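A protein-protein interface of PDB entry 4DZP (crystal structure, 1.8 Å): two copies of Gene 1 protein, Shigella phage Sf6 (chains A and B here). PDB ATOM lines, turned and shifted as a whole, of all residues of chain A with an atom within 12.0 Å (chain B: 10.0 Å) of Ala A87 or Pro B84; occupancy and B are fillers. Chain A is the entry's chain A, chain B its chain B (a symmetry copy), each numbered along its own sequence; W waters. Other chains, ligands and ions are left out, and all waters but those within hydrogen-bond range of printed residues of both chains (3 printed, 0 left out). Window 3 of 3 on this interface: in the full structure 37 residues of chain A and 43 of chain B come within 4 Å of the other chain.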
ATOM      1  N   ILE A  78     -11.077  21.374   4.548  1.00  0.00           N
ATOM      2  CA  ILE A  78     -10.537  20.018   4.483  1.00  0.00           C
ATOM      3  C   ILE A  78      -9.215  19.923   5.231  1.00  0.00           C
ATOM      4  O   ILE A  78      -8.975  18.962   5.965  1.00  0.00           O
ATOM      5  CB  ILE A  78     -10.366  19.534   3.024  1.00  0.00           C
ATOM      6  CG1 ILE A  78     -11.737  19.466   2.338  1.00  0.00           C
ATOM      7  CG2 ILE A  78      -9.680  18.180   2.988  1.00  0.00           C
ATOM      8  CD1 ILE A  78     -11.670  19.213   0.833  1.00  0.00           C
ATOM      9  N   ALA A  79      -8.352  20.922   5.039  1.00  0.00           N
ATOM     10  CA  ALA A  79      -7.046  20.934   5.699  1.00  0.00           C
ATOM     11  C   ALA A  79      -7.175  21.142   7.202  1.00  0.00           C
ATOM     12  O   ALA A  79      -6.593  20.394   7.992  1.00  0.00           O
ATOM     13  CB  ALA A  79      -6.161  22.019   5.102  1.00  0.00           C
ATOM     14  N   ASN A  81      -9.729  20.876   9.256  1.00  0.00           N
ATOM     15  CA  ASN A  81     -10.538  19.909   9.996  1.00  0.00           C
ATOM     16  C   ASN A  81     -10.104  18.455   9.830  1.00  0.00           C
ATOM     17  O   ASN A  81     -10.822  17.540  10.236  1.00  0.00           O
ATOM     18  CB  ASN A  81     -12.016  20.061   9.634  1.00  0.00           C
ATOM     19  CG  ASN A  81     -12.558  21.441   9.963  1.00  0.00           C
ATOM     20  OD1 ASN A  81     -11.985  22.179  10.764  1.00  0.00           O
ATOM     21  ND2 ASN A  81     -13.674  21.794   9.341  1.00  0.00           N
ATOM     22  N   ALA A  82      -8.936  18.230   9.233  1.00  0.00           N
ATOM     23  CA  ALA A  82      -8.462  16.867   9.023  1.00  0.00           C
ATOM     24  C   ALA A  82      -8.329  16.128  10.353  1.00  0.00           C
ATOM     25  O   ALA A  82      -7.859  16.690  11.336  1.00  0.00           O
ATOM     26  CB  ALA A  82      -7.127  16.871   8.292  1.00  0.00           C
ATOM     27  N   ILE A  83      -8.740  14.866  10.383  1.00  0.00           N
ATOM     28  CA  ILE A  83      -8.539  14.045  11.573  1.00  0.00           C
ATOM     29  C   ILE A  83      -7.053  13.730  11.732  1.00  0.00           C
ATOM     30  O   ILE A  83      -6.408  13.258  10.790  1.00  0.00           O
ATOM     31  CB  ILE A  83      -9.361  12.741  11.508  1.00  0.00           C
ATOM     32  CG1 ILE A  83     -10.862  13.057  11.496  1.00  0.00           C
ATOM     33  CG2 ILE A  83      -8.998  11.821  12.665  1.00  0.00           C
ATOM     34  CD1 ILE A  83     -11.718  11.939  10.935  1.00  0.00           C
ATOM     35  N   PRO A  84      -6.499  14.004  12.925  1.00  0.00           N
ATOM     36  CA  PRO A  84      -5.077  13.846  13.257  1.00  0.00           C
ATOM     37  C   PRO A  84      -4.629  12.387  13.323  1.00  0.00           C
ATOM     38  O   PRO A  84      -4.045  11.960  14.320  1.00  0.00           O
ATOM     39  CB  PRO A  84      -4.969  14.481  14.653  1.00  0.00           C
ATOM     40  CG  PRO A  84      -6.223  15.253  14.847  1.00  0.00           C
ATOM     41  CD  PRO A  84      -7.264  14.544  14.058  1.00  0.00           C
ATOM     42  N   ASP A  85      -4.908  11.642  12.259  1.00  0.00           N
ATOM     43  CA  ASP A  85      -4.516  10.247  12.129  1.00  0.00           C
ATOM     44  C   ASP A  85      -3.786  10.089  10.790  1.00  0.00           C
ATOM     45  O   ASP A  85      -4.169  10.712   9.806  1.00  0.00           O
ATOM     46  CB  ASP A  85      -5.768   9.367  12.184  1.00  0.00           C
ATOM     47  CG  ASP A  85      -5.534   7.972  11.646  1.00  0.00           C
ATOM     48  OD1 ASP A  85      -5.348   7.039  12.461  1.00  0.00           O
ATOM     49  OD2 ASP A  85      -5.545   7.803  10.409  1.00  0.00           O
ATOM     50  N   ALA A  86      -2.740   9.269  10.751  1.00  0.00           N
ATOM     51  CA  ALA A  86      -1.871   9.210   9.573  1.00  0.00           C
ATOM     52  C   ALA A  86      -2.624   9.061   8.247  1.00  0.00           C
ATOM     53  O   ALA A  86      -2.448   9.867   7.328  1.00  0.00           O
ATOM     54  CB  ALA A  86      -0.822   8.105   9.723  1.00  0.00           C
ATOM     55  N   ALA A  87      -3.453   8.030   8.145  1.00  0.00           N
ATOM     56  CA  ALA A  87      -4.180   7.770   6.907  1.00  0.00           C
ATOM     57  C   ALA A  87      -5.210   8.850   6.594  1.00  0.00           C
ATOM     58  O   ALA A  87      -5.438   9.175   5.425  1.00  0.00           O
ATOM     59  CB  ALA A  87      -4.842   6.398   6.949  1.00  0.00           C
ATOM     60  N   GLU A  88      -5.848   9.397   7.626  1.00  0.00           N
ATOM     61  CA  GLU A  88      -6.827  10.452   7.411  1.00  0.00           C
ATOM     62  C   GLU A  88      -6.140  11.735   6.934  1.00  0.00           C
ATOM     63  O   GLU A  88      -6.675  12.445   6.102  1.00  0.00           O
ATOM     64  CB  GLU A  88      -7.647  10.728   8.677  1.00  0.00           C
ATOM     65  CG  GLU A  88      -8.559   9.572   9.114  1.00  0.00           C
ATOM     66  CD  GLU A  88      -9.789   9.384   8.239  1.00  0.00           C
ATOM     67  OE1 GLU A  88      -9.940  10.070   7.202  1.00  0.00           O
ATOM     68  OE2 GLU A  88     -10.628   8.532   8.594  1.00  0.00           O
ATOM     69  N   VAL A  89      -4.961  12.034   7.460  1.00  0.00           N
ATOM     70  CA  VAL A  89      -4.258  13.234   7.009  1.00  0.00           C
ATOM     71  C   VAL A  89      -3.786  13.045   5.570  1.00  0.00           C
ATOM     72  O   VAL A  89      -3.881  13.971   4.758  1.00  0.00           O
ATOM     73  CB  VAL A  89      -3.074  13.626   7.917  1.00  0.00           C
ATOM     74  CG1 VAL A  89      -2.382  14.872   7.363  1.00  0.00           C
ATOM     75  CG2 VAL A  89      -3.565  13.913   9.326  1.00  0.00           C
ATOM     76  N   ALA A  90      -3.283  11.849   5.258  1.00  0.00           N
ATOM     77  CA  ALA A  90      -2.906  11.510   3.879  1.00  0.00           C
ATOM     78  C   ALA A  90      -4.094  11.632   2.924  1.00  0.00           C
ATOM     79  O   ALA A  90      -3.941  12.092   1.786  1.00  0.00           O
ATOM     80  CB  ALA A  90      -2.283  10.110   3.798  1.00  0.00           C
ATOM     81  N   LYS A  91      -5.279  11.213   3.375  1.00  0.00           N
ATOM     82  CA  LYS A  91      -6.482  11.343   2.559  1.00  0.00           C
ATOM     83  C   LYS A  91      -6.880  12.800   2.348  1.00  0.00           C
ATOM     84  O   LYS A  91      -7.216  13.214   1.239  1.00  0.00           O
ATOM     85  CB  LYS A  91      -7.658  10.588   3.192  1.00  0.00           C
ATOM     86  CG  LYS A  91      -8.925  10.675   2.376  1.00  0.00           C
ATOM     87  CD  LYS A  91     -10.046   9.812   2.967  1.00  0.00           C
ATOM     88  CE  LYS A  91     -11.367  10.102   2.264  1.00  0.00           C
ATOM     89  NZ  LYS A  91     -12.459   9.156   2.671  1.00  0.00           N
ATOM     90  N   ALA A  92      -6.828  13.578   3.421  1.00  0.00           N
ATOM     91  CA  ALA A  92      -7.130  15.005   3.348  1.00  0.00           C
ATOM     92  C   ALA A  92      -6.159  15.704   2.393  1.00  0.00           C
ATOM     93  O   ALA A  92      -6.556  16.556   1.593  1.00  0.00           O
ATOM     94  CB  ALA A  92      -7.065  15.631   4.735  1.00  0.00           C
ATOM     95  N   ARG A  93      -4.884  15.339   2.477  1.00  0.00           N
ATOM     96  CA  ARG A  93      -3.887  15.909   1.570  1.00  0.00           C
ATOM     97  C   ARG A  93      -4.203  15.561   0.119  1.00  0.00           C
ATOM     98  O   ARG A  93      -4.072  16.404  -0.767  1.00  0.00           O
ATOM     99  CB  ARG A  93      -2.487  15.420   1.928  1.00  0.00           C
ATOM    100  CG  ARG A  93      -1.380  15.981   1.046  1.00  0.00           C
ATOM    101  CD  ARG A  93      -0.033  15.482   1.518  1.00  0.00           C
ATOM    102  NE  ARG A  93       1.028  15.776   0.555  1.00  0.00           N
ATOM    103  CZ  ARG A  93       2.249  15.246   0.602  1.00  0.00           C
ATOM    104  NH1 ARG A  93       2.567  14.386   1.563  1.00  0.00           N
ATOM    105  NH2 ARG A  93       3.152  15.572  -0.315  1.00  0.00           N
ATOM    106  N   LEU A  94      -4.630  14.328  -0.131  1.00  0.00           N
ATOM    107  CA  LEU A  94      -5.027  13.937  -1.494  1.00  0.00           C
ATOM    108  C   LEU A  94      -6.264  14.721  -1.948  1.00  0.00           C
ATOM    109  O   LEU A  94      -6.355  15.155  -3.101  1.00  0.00           O
ATOM    110  CB  LEU A  94      -5.262  12.419  -1.591  1.00  0.00           C
ATOM    111  CG  LEU A  94      -5.816  11.872  -2.916  1.00  0.00           C
ATOM    112  CD1 LEU A  94      -4.854  12.116  -4.073  1.00  0.00           C
ATOM    113  CD2 LEU A  94      -6.098  10.378  -2.798  1.00  0.00           C
ATOM    114  N   ARG A  95      -7.223  14.929  -1.046  1.00  0.00           N
ATOM    115  CA  ARG A  95      -8.433  15.653  -1.422  1.00  0.00           C
ATOM    116  C   ARG A  95      -8.091  17.092  -1.782  1.00  0.00           C
ATOM    117  O   ARG A  95      -8.603  17.633  -2.756  1.00  0.00           O
ATOM    118  CB  ARG A  95      -9.453  15.627  -0.280  1.00  0.00           C
ATOM    119  CG  ARG A  95     -10.040  14.234  -0.035  1.00  0.00           C
ATOM    120  CD  ARG A  95     -11.059  14.315   1.097  1.00  0.00           C
ATOM    121  NE  ARG A  95     -12.261  15.021   0.662  1.00  0.00           N
ATOM    122  CZ  ARG A  95     -13.107  15.644   1.480  1.00  0.00           C
ATOM    123  NH1 ARG A  95     -12.873  15.676   2.783  1.00  0.00           N
ATOM    124  NH2 ARG A  95     -14.174  16.256   0.989  1.00  0.00           N
ATOM    125  N   VAL A  96      -7.202  17.694  -1.004  1.00  0.00           N
ATOM    126  CA  VAL A  96      -6.800  19.077  -1.230  1.00  0.00           C
ATOM    127  C   VAL A  96      -5.970  19.209  -2.508  1.00  0.00           C
ATOM    128  O   VAL A  96      -6.201  20.101  -3.333  1.00  0.00           O
ATOM    129  CB  VAL A  96      -5.978  19.620  -0.037  1.00  0.00           C
ATOM    130  CG1 VAL A  96      -5.322  20.958  -0.391  1.00  0.00           C
ATOM    131  CG2 VAL A  96      -6.887  19.789   1.186  1.00  0.00           C
ATOM    132  N   ASP A  97      -5.004  18.316  -2.669  1.00  0.00           N
ATOM    133  CA  ASP A  97      -4.145  18.355  -3.851  1.00  0.00           C
ATOM    134  C   ASP A  97      -4.942  18.194  -5.135  1.00  0.00           C
ATOM    135  O   ASP A  97      -4.656  18.828  -6.143  1.00  0.00           O
ATOM    136  CB  ASP A  97      -3.051  17.282  -3.753  1.00  0.00           C
ATOM    137  CG  ASP A  97      -1.980  17.633  -2.724  1.00  0.00           C
ATOM    138  OD1 ASP A  97      -1.996  18.773  -2.194  1.00  0.00           O
ATOM    139  OD2 ASP A  97      -1.116  16.771  -2.451  1.00  0.00           O
ATOM    140  N   ILE B  78     -12.442   9.546  -6.621  1.00  0.00           N
ATOM    141  CA  ILE B  78     -11.381   8.650  -6.165  1.00  0.00           C
ATOM    142  C   ILE B  78     -10.750   9.154  -4.875  1.00  0.00           C
ATOM    143  O   ILE B  78     -10.454   8.369  -3.975  1.00  0.00           O
ATOM    144  CB  ILE B  78     -10.297   8.429  -7.252  1.00  0.00           C
ATOM    145  CG1 ILE B  78     -10.928   7.730  -8.469  1.00  0.00           C
ATOM    146  CG2 ILE B  78      -9.125   7.628  -6.691  1.00  0.00           C
ATOM    147  CD1 ILE B  78     -10.023   7.665  -9.695  1.00  0.00           C
ATOM    148  N   ALA B  79     -10.541  10.465  -4.783  1.00  0.00           N
ATOM    149  CA  ALA B  79      -9.904  11.042  -3.607  1.00  0.00           C
ATOM    150  C   ALA B  79     -10.858  11.059  -2.421  1.00  0.00           C
ATOM    151  O   ALA B  79     -10.494  10.682  -1.305  1.00  0.00           O
ATOM    152  CB  ALA B  79      -9.428  12.468  -3.903  1.00  0.00           C
ATOM    153  N   ASP B  80     -12.072  11.527  -2.667  1.00  0.00           N
ATOM    154  CA  ASP B  80     -13.032  11.754  -1.591  1.00  0.00           C
ATOM    155  C   ASP B  80     -13.490  10.438  -0.958  1.00  0.00           C
ATOM    156  O   ASP B  80     -13.817  10.393   0.231  1.00  0.00           O
ATOM    157  CB  ASP B  80     -14.246  12.525  -2.121  1.00  0.00           C
ATOM    158  CG  ASP B  80     -13.937  13.985  -2.419  1.00  0.00           C
ATOM    159  OD1 ASP B  80     -12.846  14.474  -2.035  1.00  0.00           O
ATOM    160  OD2 ASP B  80     -14.806  14.650  -3.029  1.00  0.00           O
ATOM    161  N   ASN B  81     -13.514   9.375  -1.760  1.00  0.00           N
ATOM    162  CA  ASN B  81     -14.045   8.093  -1.302  1.00  0.00           C
ATOM    163  C   ASN B  81     -12.962   7.104  -0.895  1.00  0.00           C
ATOM    164  O   ASN B  81     -13.247   5.950  -0.598  1.00  0.00           O
ATOM    165  CB  ASN B  81     -14.972   7.477  -2.361  1.00  0.00           C
ATOM    166  CG  ASN B  81     -16.199   8.333  -2.638  1.00  0.00           C
ATOM    167  OD1 ASN B  81     -16.650   9.094  -1.786  1.00  0.00           O
ATOM    168  ND2 ASN B  81     -16.747   8.206  -3.835  1.00  0.00           N
ATOM    169  N   ALA B  82     -11.712   7.563  -0.873  1.00  0.00           N
ATOM    170  CA  ALA B  82     -10.596   6.714  -0.490  1.00  0.00           C
ATOM    171  C   ALA B  82     -10.802   6.080   0.890  1.00  0.00           C
ATOM    172  O   ALA B  82     -11.117   6.769   1.855  1.00  0.00           O
ATOM    173  CB  ALA B  82      -9.289   7.527  -0.509  1.00  0.00           C
ATOM    174  N   ILE B  83     -10.624   4.764   0.976  1.00  0.00           N
ATOM    175  CA  ILE B  83     -10.621   4.077   2.264  1.00  0.00           C
ATOM    176  C   ILE B  83      -9.458   4.605   3.093  1.00  0.00           C
ATOM    177  O   ILE B  83      -8.326   4.599   2.624  1.00  0.00           O
ATOM    178  CB  ILE B  83     -10.431   2.560   2.082  1.00  0.00           C
ATOM    179  CG1 ILE B  83     -11.631   1.951   1.351  1.00  0.00           C
ATOM    180  CG2 ILE B  83     -10.199   1.877   3.429  1.00  0.00           C
ATOM    181  CD1 ILE B  83     -11.444   0.490   0.980  1.00  0.00           C
ATOM    182  N   PRO B  84      -9.732   5.051   4.332  1.00  0.00           N
ATOM    183  CA  PRO B  84      -8.728   5.685   5.196  1.00  0.00           C
ATOM    184  C   PRO B  84      -7.733   4.680   5.764  1.00  0.00           C
ATOM    185  O   PRO B  84      -7.581   4.573   6.980  1.00  0.00           O
ATOM    186  CB  PRO B  84      -9.566   6.294   6.332  1.00  0.00           C
ATOM    187  CG  PRO B  84     -10.991   6.181   5.900  1.00  0.00           C
ATOM    188  CD  PRO B  84     -11.058   5.028   4.968  1.00  0.00           C
ATOM    189  N   ASP B  85      -7.075   3.945   4.876  1.00  0.00           N
ATOM    190  CA  ASP B  85      -6.007   3.028   5.244  1.00  0.00           C
ATOM    191  C   ASP B  85      -4.776   3.466   4.463  1.00  0.00           C
ATOM    192  O   ASP B  85      -4.901   3.896   3.319  1.00  0.00           O
ATOM    193  CB  ASP B  85      -6.393   1.597   4.864  1.00  0.00           C
ATOM    194  CG  ASP B  85      -5.218   0.638   4.926  1.00  0.00           C
ATOM    195  OD1 ASP B  85      -4.758   0.330   6.047  1.00  0.00           O
ATOM    196  OD2 ASP B  85      -4.762   0.186   3.852  1.00  0.00           O
ATOM    197  N   ALA B  86      -3.596   3.361   5.069  1.00  0.00           N
ATOM    198  CA  ALA B  86      -2.378   3.901   4.458  1.00  0.00           C
ATOM    199  C   ALA B  86      -2.167   3.422   3.021  1.00  0.00           C
ATOM    200  O   ALA B  86      -1.938   4.226   2.120  1.00  0.00           O
ATOM    201  CB  ALA B  86      -1.153   3.587   5.319  1.00  0.00           C
ATOM    202  N   ALA B  87      -2.246   2.115   2.805  1.00  0.00           N
ATOM    203  CA  ALA B  87      -2.056   1.547   1.470  1.00  0.00           C
ATOM    204  C   ALA B  87      -3.165   1.932   0.492  1.00  0.00           C
ATOM    205  O   ALA B  87      -2.911   2.151  -0.697  1.00  0.00           O
ATOM    206  CB  ALA B  87      -1.932   0.031   1.556  1.00  0.00           C
ATOM    207  N   GLU B  88      -4.397   1.996   0.980  1.00  0.00           N
ATOM    208  CA  GLU B  88      -5.521   2.352   0.125  1.00  0.00           C
ATOM    209  C   GLU B  88      -5.446   3.818  -0.311  1.00  0.00           C
ATOM    210  O   GLU B  88      -5.800   4.162  -1.441  1.00  0.00           O
ATOM    211  CB  GLU B  88      -6.849   2.070   0.834  1.00  0.00           C
ATOM    212  CG  GLU B  88      -7.125   0.576   1.072  1.00  0.00           C
ATOM    213  CD  GLU B  88      -7.526  -0.178  -0.190  1.00  0.00           C
ATOM    214  OE1 GLU B  88      -7.689   0.453  -1.253  1.00  0.00           O
ATOM    215  OE2 GLU B  88      -7.683  -1.417  -0.117  1.00  0.00           O
ATOM    216  N   VAL B  89      -4.987   4.677   0.590  1.00  0.00           N
ATOM    217  CA  VAL B  89      -4.822   6.087   0.251  1.00  0.00           C
ATOM    218  C   VAL B  89      -3.680   6.267  -0.744  1.00  0.00           C
ATOM    219  O   VAL B  89      -3.779   7.067  -1.679  1.00  0.00           O
ATOM    220  CB  VAL B  89      -4.606   6.952   1.495  1.00  0.00           C
ATOM    221  CG1 VAL B  89      -4.278   8.387   1.097  1.00  0.00           C
ATOM    222  CG2 VAL B  89      -5.865   6.930   2.361  1.00  0.00           C
ATOM    223  N   ALA B  90      -2.605   5.509  -0.551  1.00  0.00           N
ATOM    224  CA  ALA B  90      -1.485   5.531  -1.487  1.00  0.00           C
ATOM    225  C   ALA B  90      -1.909   5.087  -2.881  1.00  0.00           C
ATOM    226  O   ALA B  90      -1.463   5.657  -3.890  1.00  0.00           O
ATOM    227  CB  ALA B  90      -0.328   4.672  -0.971  1.00  0.00           C
ATOM    228  N   ALA B  92      -5.080   5.282  -4.075  1.00  0.00           N
ATOM    229  CA  ALA B  92      -5.959   6.337  -4.568  1.00  0.00           C
ATOM    230  C   ALA B  92      -5.123   7.476  -5.140  1.00  0.00           C
ATOM    231  O   ALA B  92      -5.424   7.999  -6.210  1.00  0.00           O
ATOM    232  CB  ALA B  92      -6.865   6.848  -3.447  1.00  0.00           C
ATOM    233  N   ARG B  93      -4.078   7.849  -4.415  1.00  0.00           N
ATOM    234  CA  ARG B  93      -3.151   8.886  -4.875  1.00  0.00           C
ATOM    235  C   ARG B  93      -2.538   8.522  -6.214  1.00  0.00           C
ATOM    236  O   ARG B  93      -2.505   9.334  -7.136  1.00  0.00           O
ATOM    237  CB  ARG B  93      -2.042   9.108  -3.848  1.00  0.00           C
ATOM    238  CG  ARG B  93      -1.126  10.276  -4.184  1.00  0.00           C
ATOM    239  CD  ARG B  93       0.001  10.404  -3.170  1.00  0.00           C
ATOM    240  NE  ARG B  93       0.943  11.447  -3.555  1.00  0.00           N
ATOM    241  CZ  ARG B  93       2.134  11.624  -2.992  1.00  0.00           C
ATOM    242  NH1 ARG B  93       2.537  10.822  -2.013  1.00  0.00           N
ATOM    243  NH2 ARG B  93       2.926  12.604  -3.413  1.00  0.00           N
HETATM  244  O   HOH W   1      -7.082   5.503   9.733  1.00  0.00           O
HETATM  245  O   HOH W   2     -15.291   9.494   2.845  1.00  0.00           O
HETATM  246  O   HOH W   3     -14.116  12.697   1.755  1.00  0.00           O
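The side-chain amino group of Lys A91 sits at hydrogen-bond distance from the backbone carbonyl oxygen of Asp B80, at 3.1 Å. NZ of Lys A91 sits at hydrogen-bond distance from O of Ala B82, at 2.9 Å. The guanidinium group of Arg A95 lies within salt-bridge range of the side-chain carboxylate of Asp B80, at 2.8 Å.
The backbone NH of Ala A87 lies within hydrogen-bond range of the side-chain carboxylate of Asp A85, 3.1 Å away. The backbone NH (N) of Glu A88 lies within hydrogen-bond range of the side-chain carboxylate (OD2) of Asp A85 (3.2 Å). The backbone NH of Ala B87 lies close to the side-chain carboxylate of Asp B85 (3.3 Å). OD2 of Asp B85 is in hydrogen-bond range of N of Glu B88.
Among the printed residues, pairs that only touch across the chains: Ala A87 with Pro B84 (3.3 Å), Ala A87 with Asp B85 (3.8 Å), Ala A87 with Ala B86 (3.8 Å), Ala A87 with Val B89 (3.8 Å), Glu A88 with Pro B84 (3.4 Å), Ala A90 with Val B89 (3.7 Å), Lys A91 with Ala B79 (3.7 Å), Lys A91 with Val B89 (3.8 Å), Leu A94 with Ala B79 (3.8 Å), Leu A94 with Ala B92 (3.7 Å), Leu A94 with Arg B93 (3.6 Å) and Arg A95 with Ala B79 (3.8 Å).
No residue of chain B comes within 4 Å of Asp A85. No residue of chain B comes within 4 Å of Ala A86. Ala A87 touches just these residues of chain B: Pro B84 (3.3 Å), Asp B85 (3.8 Å), Ala B86 (3.8 Å) and Val B89 (3.8 Å). Glu A88 touches one residue of chain B. Ala A90 touches just one residue of chain B: Val B89 (3.7 Å). Printed residues of chain B within 4 Å of Arg A95: Ala B79 and Asp B80. Of the printed residues of chain A, Ala B79 touches Lys A91 (3.7 Å), Leu A94 (3.8 Å) and Arg A95 (3.8 Å). Of the printed residues of chain A, Asp B80 touches Lys A91 (3.1 Å) and Arg A95 (2.8 Å). Of chain A, only Lys A91 (2.9 Å) comes within 4 Å of Ala B82. Ile B83 touches none of the printed residues of chain A. Pro B84 touches just these residues of chain A: Ala A87 (3.3 Å) and Glu A88 (3.4 Å). Of chain A, only Ala A87 (3.8 Å) comes within 4 Å of Asp B85. Printed residues of chain A within 4 Å of Ala B86: Ala A87 (3.8 Å). Of chain A, only Ala A87, Ala A90 and Lys A91 come within 4 Å of Val B89. Of the printed residues of chain A, Ala B92 touches Leu A94 (3.7 Å). Printed residues of chain A within 4 Å of Arg B93: Leu A94 (3.6 Å). The nearest residue of chain B that does not touch Ala A87 is Ile B83 (5.8 Å). The nearest printed residue of chain B that does not touch Lys A91 is Asn B81 (4.1 Å).
Of the 15 printed residues of chain B, 9 touch a printed residue of chain A. Hydrophobic or aromatic side chains of chain B within 4 Å of the printed part of chain A: Ala B79, Pro B84, Val B89 and Ala B92. Printed residues of chain A that touch a printed residue of chain B: Ala A87, Glu A88, Ala A90, Lys A91, Leu A94 and Arg A95. Hydrophobic or aromatic side chains of chain A within 4 Å of the printed part of chain B: Ala A87, Ala A90 and Leu A94. Among the printed residues, 15 pairs touch across the chains. Among the printed residues, Asp or Glu carboxylates within 4 Å of a Lys or Arg side-chain nitrogen of the other chain: Arg A95 with Asp B80.
Ala A87 touches Ala B86, but with the chains exchanged Ala A86 does not touch Ala B87 (8.8 Å). Ala A87 touches Val B89, but with the chains exchanged Val A89 does not touch Ala B87 (11.3 Å). Glu A88 touches Pro B84, but with the chains exchanged Pro A84 does not touch Glu B88 (16.1 Å). Ala A90 touches Val B89, but with the chains exchanged Val A89 does not touch Ala B90 (9.8 Å). Positions printed for both chains: 78, 79, 81, 82, 83, 84, 85, 86, 87, 88, 89, 90, 92 and 93.
Water W3 lies within hydrogen-bond range of O of Asp B80 (2.8 Å) and NE of Arg A95 (3.2 Å). Water W1 bridges OD2 of Asp A85 and O of Pro B84. Water W2 bridges the side-chain amino group (NZ) of Lys A91 (2.9 Å) and the backbone carbonyl oxygen (O) of Asp B80 (3.1 Å).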
